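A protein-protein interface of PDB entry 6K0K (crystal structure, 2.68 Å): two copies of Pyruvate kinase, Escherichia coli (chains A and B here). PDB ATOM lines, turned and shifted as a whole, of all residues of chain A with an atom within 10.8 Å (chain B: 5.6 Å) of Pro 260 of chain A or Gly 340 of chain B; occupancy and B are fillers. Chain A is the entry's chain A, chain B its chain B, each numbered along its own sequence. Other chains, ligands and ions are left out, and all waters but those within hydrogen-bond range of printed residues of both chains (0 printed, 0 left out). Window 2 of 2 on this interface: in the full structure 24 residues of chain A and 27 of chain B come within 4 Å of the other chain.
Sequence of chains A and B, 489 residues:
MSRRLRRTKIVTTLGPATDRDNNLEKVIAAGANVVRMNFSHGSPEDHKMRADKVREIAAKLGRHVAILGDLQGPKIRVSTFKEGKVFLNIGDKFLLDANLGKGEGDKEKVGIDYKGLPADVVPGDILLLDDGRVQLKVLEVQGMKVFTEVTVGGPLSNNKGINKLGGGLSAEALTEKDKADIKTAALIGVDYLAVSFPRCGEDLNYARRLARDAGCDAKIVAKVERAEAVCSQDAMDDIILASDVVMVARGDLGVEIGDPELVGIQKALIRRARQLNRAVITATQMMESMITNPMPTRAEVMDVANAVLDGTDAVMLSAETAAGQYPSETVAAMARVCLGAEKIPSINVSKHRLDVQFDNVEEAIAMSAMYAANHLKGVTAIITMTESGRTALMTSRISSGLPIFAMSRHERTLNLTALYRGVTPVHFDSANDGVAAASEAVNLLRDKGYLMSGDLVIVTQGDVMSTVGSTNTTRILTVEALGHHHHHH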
ATOM      1  N   LEU A 128      26.246  10.589  -0.588  1.00  0.00           N
ATOM      2  CA  LEU A 128      27.219  10.745  -1.659  1.00  0.00           C
ATOM      3  C   LEU A 128      28.605  10.923  -1.046  1.00  0.00           C
ATOM      4  O   LEU A 128      28.825  11.817  -0.216  1.00  0.00           O
ATOM      5  CB  LEU A 128      26.859  11.917  -2.573  1.00  0.00           C
ATOM      6  CG  LEU A 128      25.511  11.867  -3.304  1.00  0.00           C
ATOM      7  CD1 LEU A 128      24.389  12.505  -2.488  1.00  0.00           C
ATOM      8  CD2 LEU A 128      25.630  12.548  -4.661  1.00  0.00           C
ATOM      9  N   ASP A 131      31.926  13.772  -3.411  1.00  0.00           N
ATOM     10  CA  ASP A 131      31.186  14.598  -4.364  1.00  0.00           C
ATOM     11  C   ASP A 131      30.262  13.798  -5.280  1.00  0.00           C
ATOM     12  O   ASP A 131      29.801  14.315  -6.299  1.00  0.00           O
ATOM     13  CB  ASP A 131      32.144  15.438  -5.204  1.00  0.00           C
ATOM     14  CG  ASP A 131      33.145  16.159  -4.360  1.00  0.00           C
ATOM     15  OD1 ASP A 131      32.732  17.106  -3.649  1.00  0.00           O
ATOM     16  OD2 ASP A 131      34.332  15.752  -4.386  1.00  0.00           O
ATOM     17  N   LEU A 165      22.093  13.559   0.385  1.00  0.00           N
ATOM     18  CA  LEU A 165      21.218  14.134  -0.641  1.00  0.00           C
ATOM     19  C   LEU A 165      20.120  14.951   0.023  1.00  0.00           C
ATOM     20  O   LEU A 165      19.388  14.442   0.881  1.00  0.00           O
ATOM     21  CB  LEU A 165      20.610  13.025  -1.510  1.00  0.00           C
ATOM     22  CG  LEU A 165      20.049  13.335  -2.920  1.00  0.00           C
ATOM     23  CD1 LEU A 165      18.861  14.303  -2.919  1.00  0.00           C
ATOM     24  CD2 LEU A 165      21.122  13.837  -3.884  1.00  0.00           C
ATOM     25  N   VAL A 230      19.570  27.333   1.178  1.00  0.00           N
ATOM     26  CA  VAL A 230      19.036  27.845  -0.077  1.00  0.00           C
ATOM     27  C   VAL A 230      17.642  27.284  -0.382  1.00  0.00           C
ATOM     28  O   VAL A 230      17.168  27.390  -1.509  1.00  0.00           O
ATOM     29  CB  VAL A 230      20.020  27.585  -1.238  1.00  0.00           C
ATOM     30  CG1 VAL A 230      21.340  28.321  -1.005  1.00  0.00           C
ATOM     31  CG2 VAL A 230      20.282  26.104  -1.411  1.00  0.00           C
ATOM     32  N   ARG A 250      30.630  25.815  -4.011  1.00  0.00           N
ATOM     33  CA  ARG A 250      29.841  25.022  -4.946  1.00  0.00           C
ATOM     34  C   ARG A 250      30.005  23.507  -4.783  1.00  0.00           C
ATOM     35  O   ARG A 250      29.087  22.768  -5.161  1.00  0.00           O
ATOM     36  CB  ARG A 250      30.176  25.462  -6.377  1.00  0.00           C
ATOM     37  CG  ARG A 250      30.229  26.995  -6.511  1.00  0.00           C
ATOM     38  CD  ARG A 250      30.332  27.442  -7.948  1.00  0.00           C
ATOM     39  NE  ARG A 250      31.679  27.328  -8.487  1.00  0.00           N
ATOM     40  CZ  ARG A 250      31.963  27.480  -9.769  1.00  0.00           C
ATOM     41  NH1 ARG A 250      30.984  27.744 -10.620  1.00  0.00           N
ATOM     42  NH2 ARG A 250      33.214  27.366 -10.198  1.00  0.00           N
ATOM     43  N   GLY A 251      31.111  23.026  -4.207  1.00  0.00           N
ATOM     44  CA  GLY A 251      31.360  21.602  -4.075  1.00  0.00           C
ATOM     45  C   GLY A 251      30.285  20.860  -3.308  1.00  0.00           C
ATOM     46  O   GLY A 251      29.464  20.127  -3.891  1.00  0.00           O
ATOM     47  N   LEU A 253      27.620  22.106  -1.773  1.00  0.00           N
ATOM     48  CA  LEU A 253      26.255  22.584  -2.019  1.00  0.00           C
ATOM     49  C   LEU A 253      25.669  21.968  -3.285  1.00  0.00           C
ATOM     50  O   LEU A 253      24.480  21.629  -3.337  1.00  0.00           O
ATOM     51  CB  LEU A 253      26.235  24.117  -2.102  1.00  0.00           C
ATOM     52  CG  LEU A 253      24.928  24.806  -2.537  1.00  0.00           C
ATOM     53  CD1 LEU A 253      23.803  24.542  -1.540  1.00  0.00           C
ATOM     54  CD2 LEU A 253      25.102  26.320  -2.788  1.00  0.00           C
ATOM     55  N   GLY A 254      26.497  21.810  -4.317  1.00  0.00           N
ATOM     56  CA  GLY A 254      26.040  21.156  -5.522  1.00  0.00           C
ATOM     57  C   GLY A 254      25.883  19.664  -5.355  1.00  0.00           C
ATOM     58  O   GLY A 254      25.081  19.049  -6.054  1.00  0.00           O
ATOM     59  N   VAL A 255      26.655  19.053  -4.452  1.00  0.00           N
ATOM     60  CA  VAL A 255      26.432  17.625  -4.214  1.00  0.00           C
ATOM     61  C   VAL A 255      25.118  17.383  -3.475  1.00  0.00           C
ATOM     62  O   VAL A 255      24.442  16.375  -3.716  1.00  0.00           O
ATOM     63  CB  VAL A 255      27.621  17.008  -3.460  1.00  0.00           C
ATOM     64  CG1 VAL A 255      27.351  15.539  -3.177  1.00  0.00           C
ATOM     65  CG2 VAL A 255      28.870  17.163  -4.282  1.00  0.00           C
ATOM     66  N   GLU A 256      24.733  18.281  -2.567  1.00  0.00           N
ATOM     67  CA  GLU A 256      23.534  18.043  -1.765  1.00  0.00           C
ATOM     68  C   GLU A 256      22.264  18.232  -2.589  1.00  0.00           C
ATOM     69  O   GLU A 256      21.478  17.291  -2.757  1.00  0.00           O
ATOM     70  CB  GLU A 256      23.538  18.943  -0.535  1.00  0.00           C
ATOM     71  CG  GLU A 256      24.656  18.593   0.434  1.00  0.00           C
ATOM     72  CD  GLU A 256      24.463  19.191   1.829  1.00  0.00           C
ATOM     73  OE1 GLU A 256      23.478  19.935   2.064  1.00  0.00           O
ATOM     74  OE2 GLU A 256      25.314  18.902   2.692  1.00  0.00           O
ATOM     75  N   ILE A 257      22.037  19.445  -3.104  1.00  0.00           N
ATOM     76  CA  ILE A 257      21.014  19.674  -4.125  1.00  0.00           C
ATOM     77  C   ILE A 257      21.626  19.196  -5.432  1.00  0.00           C
ATOM     78  O   ILE A 257      22.753  18.696  -5.437  1.00  0.00           O
ATOM     79  CB  ILE A 257      20.586  21.149  -4.182  1.00  0.00           C
ATOM     80  CG1 ILE A 257      21.710  22.016  -4.740  1.00  0.00           C
ATOM     81  CG2 ILE A 257      20.283  21.643  -2.787  1.00  0.00           C
ATOM     82  CD1 ILE A 257      21.393  23.527  -4.758  1.00  0.00           C
ATOM     83  N   GLY A 258      20.921  19.312  -6.546  1.00  0.00           N
ATOM     84  CA  GLY A 258      21.505  18.859  -7.802  1.00  0.00           C
ATOM     85  C   GLY A 258      22.576  19.801  -8.327  1.00  0.00           C
ATOM     86  O   GLY A 258      22.523  21.018  -8.130  1.00  0.00           O
ATOM     87  N   ASP A 259      23.572  19.231  -9.013  1.00  0.00           N
ATOM     88  CA  ASP A 259      24.526  20.066  -9.746  1.00  0.00           C
ATOM     89  C   ASP A 259      23.859  20.965 -10.788  1.00  0.00           C
ATOM     90  O   ASP A 259      24.276  22.132 -10.915  1.00  0.00           O
ATOM     91  CB  ASP A 259      25.599  19.193 -10.409  1.00  0.00           C
ATOM     92  CG  ASP A 259      26.964  19.312  -9.736  1.00  0.00           C
ATOM     93  OD1 ASP A 259      27.090  20.069  -8.744  1.00  0.00           O
ATOM     94  OD2 ASP A 259      27.910  18.636 -10.198  1.00  0.00           O
ATOM     95  N   PRO A 260      22.860  20.517 -11.560  1.00  0.00           N
ATOM     96  CA  PRO A 260      22.097  21.495 -12.354  1.00  0.00           C
ATOM     97  C   PRO A 260      21.448  22.599 -11.524  1.00  0.00           C
ATOM     98  O   PRO A 260      21.480  23.758 -11.947  1.00  0.00           O
ATOM     99  CB  PRO A 260      21.065  20.623 -13.077  1.00  0.00           C
ATOM    100  CG  PRO A 260      21.767  19.322 -13.248  1.00  0.00           C
ATOM    101  CD  PRO A 260      22.553  19.133 -11.977  1.00  0.00           C
ATOM    102  N   GLU A 261      20.866  22.302 -10.362  1.00  0.00           N
ATOM    103  CA  GLU A 261      20.181  23.369  -9.630  1.00  0.00           C
ATOM    104  C   GLU A 261      21.158  24.373  -9.016  1.00  0.00           C
ATOM    105  O   GLU A 261      20.759  25.496  -8.653  1.00  0.00           O
ATOM    106  CB  GLU A 261      19.256  22.752  -8.574  1.00  0.00           C
ATOM    107  CG  GLU A 261      18.400  21.571  -9.122  1.00  0.00           C
ATOM    108  CD  GLU A 261      17.222  22.000 -10.032  1.00  0.00           C
ATOM    109  OE1 GLU A 261      16.621  23.063  -9.768  1.00  0.00           O
ATOM    110  OE2 GLU A 261      16.892  21.272 -11.011  1.00  0.00           O
ATOM    111  N   LEU A 262      22.438  24.021  -8.991  1.00  0.00           N
ATOM    112  CA  LEU A 262      23.483  24.913  -8.508  1.00  0.00           C
ATOM    113  C   LEU A 262      23.578  26.205  -9.324  1.00  0.00           C
ATOM    114  O   LEU A 262      23.883  27.256  -8.764  1.00  0.00           O
ATOM    115  CB  LEU A 262      24.826  24.170  -8.524  1.00  0.00           C
ATOM    116  CG  LEU A 262      26.069  24.654  -7.763  1.00  0.00           C
ATOM    117  CD1 LEU A 262      26.975  25.525  -8.631  1.00  0.00           C
ATOM    118  CD2 LEU A 262      25.646  25.376  -6.479  1.00  0.00           C
ATOM    119  N   VAL A 263      23.386  26.154 -10.646  1.00  0.00           N
ATOM    120  CA  VAL A 263      23.613  27.357 -11.452  1.00  0.00           C
ATOM    121  C   VAL A 263      22.603  28.442 -11.090  1.00  0.00           C
ATOM    122  O   VAL A 263      22.954  29.616 -10.869  1.00  0.00           O
ATOM    123  CB  VAL A 263      23.548  27.042 -12.958  1.00  0.00           C
ATOM    124  CG1 VAL A 263      24.034  28.266 -13.740  1.00  0.00           C
ATOM    125  CG2 VAL A 263      24.375  25.833 -13.307  1.00  0.00           C
ATOM    126  N   GLY A 264      21.322  28.073 -11.073  1.00  0.00           N
ATOM    127  CA  GLY A 264      20.324  28.986 -10.568  1.00  0.00           C
ATOM    128  C   GLY A 264      20.658  29.489  -9.182  1.00  0.00           C
ATOM    129  O   GLY A 264      20.587  30.692  -8.918  1.00  0.00           O
ATOM    130  N   ILE A 265      21.057  28.580  -8.281  1.00  0.00           N
ATOM    131  CA  ILE A 265      21.294  28.979  -6.890  1.00  0.00           C
ATOM    132  C   ILE A 265      22.463  29.960  -6.778  1.00  0.00           C
ATOM    133  O   ILE A 265      22.443  30.879  -5.946  1.00  0.00           O
ATOM    134  CB  ILE A 265      21.505  27.738  -6.002  1.00  0.00           C
ATOM    135  CG1 ILE A 265      20.191  26.992  -5.865  1.00  0.00           C
ATOM    136  CG2 ILE A 265      21.917  28.145  -4.598  1.00  0.00           C
ATOM    137  CD1 ILE A 265      19.108  27.835  -5.251  1.00  0.00           C
ATOM    138  N   GLN A 266      23.504  29.770  -7.583  1.00  0.00           N
ATOM    139  CA  GLN A 266      24.649  30.673  -7.555  1.00  0.00           C
ATOM    140  C   GLN A 266      24.233  32.059  -8.023  1.00  0.00           C
ATOM    141  O   GLN A 266      24.497  33.069  -7.355  1.00  0.00           O
ATOM    142  CB  GLN A 266      25.785  30.127  -8.439  1.00  0.00           C
ATOM    143  CG  GLN A 266      26.988  31.066  -8.584  1.00  0.00           C
ATOM    144  CD  GLN A 266      28.010  30.609  -9.630  1.00  0.00           C
ATOM    145  OE1 GLN A 266      28.613  29.536  -9.514  1.00  0.00           O
ATOM    146  NE2 GLN A 266      28.218  31.439 -10.656  1.00  0.00           N
ATOM    147  N   LYS A 267      23.581  32.117  -9.182  1.00  0.00           N
ATOM    148  CA  LYS A 267      23.106  33.395  -9.668  1.00  0.00           C
ATOM    149  C   LYS A 267      22.216  34.077  -8.626  1.00  0.00           C
ATOM    150  O   LYS A 267      22.338  35.292  -8.372  1.00  0.00           O
ATOM    151  CB  LYS A 267      22.411  33.183 -11.018  1.00  0.00           C
ATOM    152  CG  LYS A 267      23.406  32.966 -12.164  1.00  0.00           C
ATOM    153  CD  LYS A 267      22.962  31.922 -13.185  1.00  0.00           C
ATOM    154  CE  LYS A 267      23.329  32.327 -14.617  1.00  0.00           C
ATOM    155  NZ  LYS A 267      24.751  32.213 -14.980  1.00  0.00           N
ATOM    156  N   ALA A 268      21.384  33.298  -7.947  1.00  0.00           N
ATOM    157  CA  ALA A 268      20.458  33.881  -6.989  1.00  0.00           C
ATOM    158  C   ALA A 268      21.190  34.434  -5.766  1.00  0.00           C
ATOM    159  O   ALA A 268      20.848  35.524  -5.286  1.00  0.00           O
ATOM    160  CB  ALA A 268      19.406  32.842  -6.577  1.00  0.00           C
ATOM    161  N   ARG B   4       7.284  17.657 -17.573  1.00  0.00           N
ATOM    162  CA  ARG B   4       8.011  18.752 -18.210  1.00  0.00           C
ATOM    163  C   ARG B   4       9.052  18.212 -19.186  1.00  0.00           C
ATOM    164  O   ARG B   4       9.837  17.323 -18.843  1.00  0.00           O
ATOM    165  CB  ARG B   4       8.688  19.615 -17.149  1.00  0.00           C
ATOM    166  CG  ARG B   4       9.155  20.966 -17.636  1.00  0.00           C
ATOM    167  CD  ARG B   4       9.897  21.748 -16.536  1.00  0.00           C
ATOM    168  NE  ARG B   4      11.351  21.716 -16.728  1.00  0.00           N
ATOM    169  CZ  ARG B   4      12.224  21.115 -15.916  1.00  0.00           C
ATOM    170  NH1 ARG B   4      11.811  20.499 -14.813  1.00  0.00           N
ATOM    171  NH2 ARG B   4      13.521  21.132 -16.209  1.00  0.00           N
ATOM    172  N   VAL B 301      29.255  21.393 -16.557  1.00  0.00           N
ATOM    173  CA  VAL B 301      27.848  21.630 -16.266  1.00  0.00           C
ATOM    174  C   VAL B 301      27.541  23.121 -16.307  1.00  0.00           C
ATOM    175  O   VAL B 301      26.489  23.546 -16.804  1.00  0.00           O
ATOM    176  CB  VAL B 301      27.497  21.012 -14.899  1.00  0.00           C
ATOM    177  CG1 VAL B 301      26.051  21.344 -14.480  1.00  0.00           C
ATOM    178  CG2 VAL B 301      27.720  19.530 -14.941  1.00  0.00           C
ATOM    179  N   ALA B 335      21.348  15.984 -20.966  1.00  0.00           N
ATOM    180  CA  ALA B 335      19.911  16.224 -20.865  1.00  0.00           C
ATOM    181  C   ALA B 335      19.517  16.711 -19.473  1.00  0.00           C
ATOM    182  O   ALA B 335      18.733  17.662 -19.335  1.00  0.00           O
ATOM    183  CB  ALA B 335      19.139  14.958 -21.224  1.00  0.00           C
ATOM    184  N   ARG B 336      20.014  16.043 -18.422  1.00  0.00           N
ATOM    185  CA  ARG B 336      19.653  16.473 -17.075  1.00  0.00           C
ATOM    186  C   ARG B 336      20.119  17.900 -16.809  1.00  0.00           C
ATOM    187  O   ARG B 336      19.392  18.706 -16.212  1.00  0.00           O
ATOM    188  CB  ARG B 336      20.234  15.515 -16.041  1.00  0.00           C
ATOM    189  CG  ARG B 336      19.409  14.218 -15.882  1.00  0.00           C
ATOM    190  CD  ARG B 336      19.922  13.370 -14.720  1.00  0.00           C
ATOM    191  NE  ARG B 336      21.333  13.037 -14.900  1.00  0.00           N
ATOM    192  CZ  ARG B 336      21.768  11.999 -15.612  1.00  0.00           C
ATOM    193  NH1 ARG B 336      20.892  11.184 -16.205  1.00  0.00           N
ATOM    194  NH2 ARG B 336      23.077  11.779 -15.729  1.00  0.00           N
ATOM    195  N   VAL B 337      21.318  18.241 -17.269  1.00  0.00           N
ATOM    196  CA  VAL B 337      21.776  19.613 -17.094  1.00  0.00           C
ATOM    197  C   VAL B 337      20.842  20.571 -17.814  1.00  0.00           C
ATOM    198  O   VAL B 337      20.440  21.599 -17.254  1.00  0.00           O
ATOM    199  CB  VAL B 337      23.228  19.778 -17.572  1.00  0.00           C
ATOM    200  CG1 VAL B 337      23.639  21.260 -17.503  1.00  0.00           C
ATOM    201  CG2 VAL B 337      24.174  18.888 -16.756  1.00  0.00           C
ATOM    202  N   CYS B 338      20.475  20.248 -19.060  1.00  0.00           N
ATOM    203  CA  CYS B 338      19.567  21.116 -19.810  1.00  0.00           C
ATOM    204  C   CYS B 338      18.237  21.308 -19.071  1.00  0.00           C
ATOM    205  O   CYS B 338      17.775  22.440 -18.876  1.00  0.00           O
ATOM    206  CB  CYS B 338      19.358  20.550 -21.221  1.00  0.00           C
ATOM    207  SG  CYS B 338      20.770  20.800 -22.356  1.00  0.00           S
ATOM    208  N   LEU B 339      17.617  20.213 -18.634  1.00  0.00           N
ATOM    209  CA  LEU B 339      16.363  20.334 -17.896  1.00  0.00           C
ATOM    210  C   LEU B 339      16.536  21.196 -16.663  1.00  0.00           C
ATOM    211  O   LEU B 339      15.683  22.037 -16.368  1.00  0.00           O
ATOM    212  CB  LEU B 339      15.828  18.965 -17.496  1.00  0.00           C
ATOM    213  CG  LEU B 339      15.133  18.160 -18.580  1.00  0.00           C
ATOM    214  CD1 LEU B 339      15.343  16.700 -18.285  1.00  0.00           C
ATOM    215  CD2 LEU B 339      13.648  18.500 -18.620  1.00  0.00           C
ATOM    216  N   GLY B 340      17.629  21.006 -15.926  1.00  0.00           N
ATOM    217  CA  GLY B 340      17.810  21.776 -14.710  1.00  0.00           C
ATOM    218  C   GLY B 340      17.923  23.251 -15.007  1.00  0.00           C
ATOM    219  O   GLY B 340      17.274  24.079 -14.370  1.00  0.00           O
ATOM    220  N   ALA B 341      18.716  23.591 -16.024  1.00  0.00           N
ATOM    221  CA  ALA B 341      18.918  24.986 -16.385  1.00  0.00           C
ATOM    222  C   ALA B 341      17.637  25.630 -16.898  1.00  0.00           C
ATOM    223  O   ALA B 341      17.426  26.835 -16.713  1.00  0.00           O
ATOM    224  CB  ALA B 341      20.020  25.087 -17.432  1.00  0.00           C
ATOM    225  N   GLU B 342      16.763  24.851 -17.533  1.00  0.00           N
ATOM    226  CA  GLU B 342      15.561  25.446 -18.109  1.00  0.00           C
ATOM    227  C   GLU B 342      14.558  25.935 -17.065  1.00  0.00           C
ATOM    228  O   GLU B 342      13.646  26.684 -17.429  1.00  0.00           O
ATOM    229  CB  GLU B 342      14.907  24.450 -19.067  1.00  0.00           C
ATOM    230  CG  GLU B 342      15.727  24.249 -20.332  1.00  0.00           C
ATOM    231  CD  GLU B 342      15.363  22.989 -21.104  1.00  0.00           C
ATOM    232  OE1 GLU B 342      14.278  22.409 -20.839  1.00  0.00           O
ATOM    233  OE2 GLU B 342      16.163  22.595 -21.982  1.00  0.00           O
ATOM    234  N   LYS B 343      14.701  25.570 -15.780  1.00  0.00           N
ATOM    235  CA  LYS B 343      13.786  26.110 -14.768  1.00  0.00           C
ATOM    236  C   LYS B 343      14.098  27.546 -14.393  1.00  0.00           C
ATOM    237  O   LYS B 343      13.235  28.219 -13.819  1.00  0.00           O
ATOM    238  CB  LYS B 343      13.791  25.270 -13.489  1.00  0.00           C
ATOM    239  CG  LYS B 343      13.202  23.878 -13.619  1.00  0.00           C
ATOM    240  CD  LYS B 343      12.613  23.373 -12.285  1.00  0.00           C
ATOM    241  CE  LYS B 343      13.682  22.936 -11.265  1.00  0.00           C
ATOM    242  NZ  LYS B 343      13.059  22.426 -10.007  1.00  0.00           N
ATOM    243  N   ILE B 344      15.294  28.041 -14.697  1.00  0.00           N
ATOM    244  CA  ILE B 344      15.667  29.402 -14.285  1.00  0.00           C
ATOM    245  C   ILE B 344      14.759  30.441 -14.948  1.00  0.00           C
ATOM    246  O   ILE B 344      14.653  30.484 -16.184  1.00  0.00           O
ATOM    247  CB  ILE B 344      17.148  29.671 -14.568  1.00  0.00           C
ATOM    248  CG1 ILE B 344      18.005  28.680 -13.788  1.00  0.00           C
ATOM    249  CG2 ILE B 344      17.512  31.078 -14.187  1.00  0.00           C
ATOM    250  CD1 ILE B 344      19.488  28.655 -14.231  1.00  0.00           C
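NZ of Lys 343 of chain B lies within salt-bridge range of OE1 of Glu 261 of chain A.
Among the printed residues, pairs that only touch across the chains: Gly 264 of chain A with Ile 344 of chain B (3.7 Å), Pro 260 of chain A with Gly 340 of chain B (3.8 Å), Glu 261 of chain A with Gly 340 of chain B (3.8 Å), Pro 260 of chain A with Arg 336 of chain B (3.8 Å) and Pro 260 of chain A with Val 337 of chain B (3.9 Å).
Val 255 of chain A touches none of the printed residues of chain B.
Pro 260 of chain A touches just these residues of chain B: Arg 336 (3.8 Å), Val 337 (3.9 Å) and Gly 340 (3.8 Å).
Of the printed residues of chain B, Glu 261 of chain A touches Gly 340 and Lys 343.
Of the printed residues of chain B, Gly 264 of chain A touches Ile 344.
Of the printed residues of chain A, Arg 336 of chain B touches Pro 260 (3.8 Å).
Gly 340 of chain B touches just these residues of chain A: Pro 260 and Glu 261.
No residue of chain A comes within 4 Å of Ala 341 of chain B.
No residue of chain A comes within 4 Å of Glu 342 of chain B.
Lys 343 of chain B touches one residue of chain A.
Of the printed residues of chain A, Ile 344 of chain B touches Gly 264 (3.7 Å).
The nearest residue of chain A that does not touch Gly 340 of chain B is Gly 264 of chain A (6.6 Å).
The nearest printed residue of chain B that does not touch Gly 264 of chain A is Gly 340 of chain B (6.6 Å).
Hydrophobic or aromatic side chains of chain B within 4 Å of the printed part of chain A: Ile 344.
Of the 22 printed residues of chain A, 3 touch a printed residue of chain B.
Among the printed residues, 6 pairs touch across the chains.
Among the printed residues, Asp or Glu carboxylates within 4 Å of a Lys or Arg side-chain nitrogen of the other chain: Glu 261 of chain A with Lys 343 of chain B.
No position is printed for both chains.
Of the 6 pairs that touch across the chains among the printed residues, none has its exchanged pair printed and touching as well.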
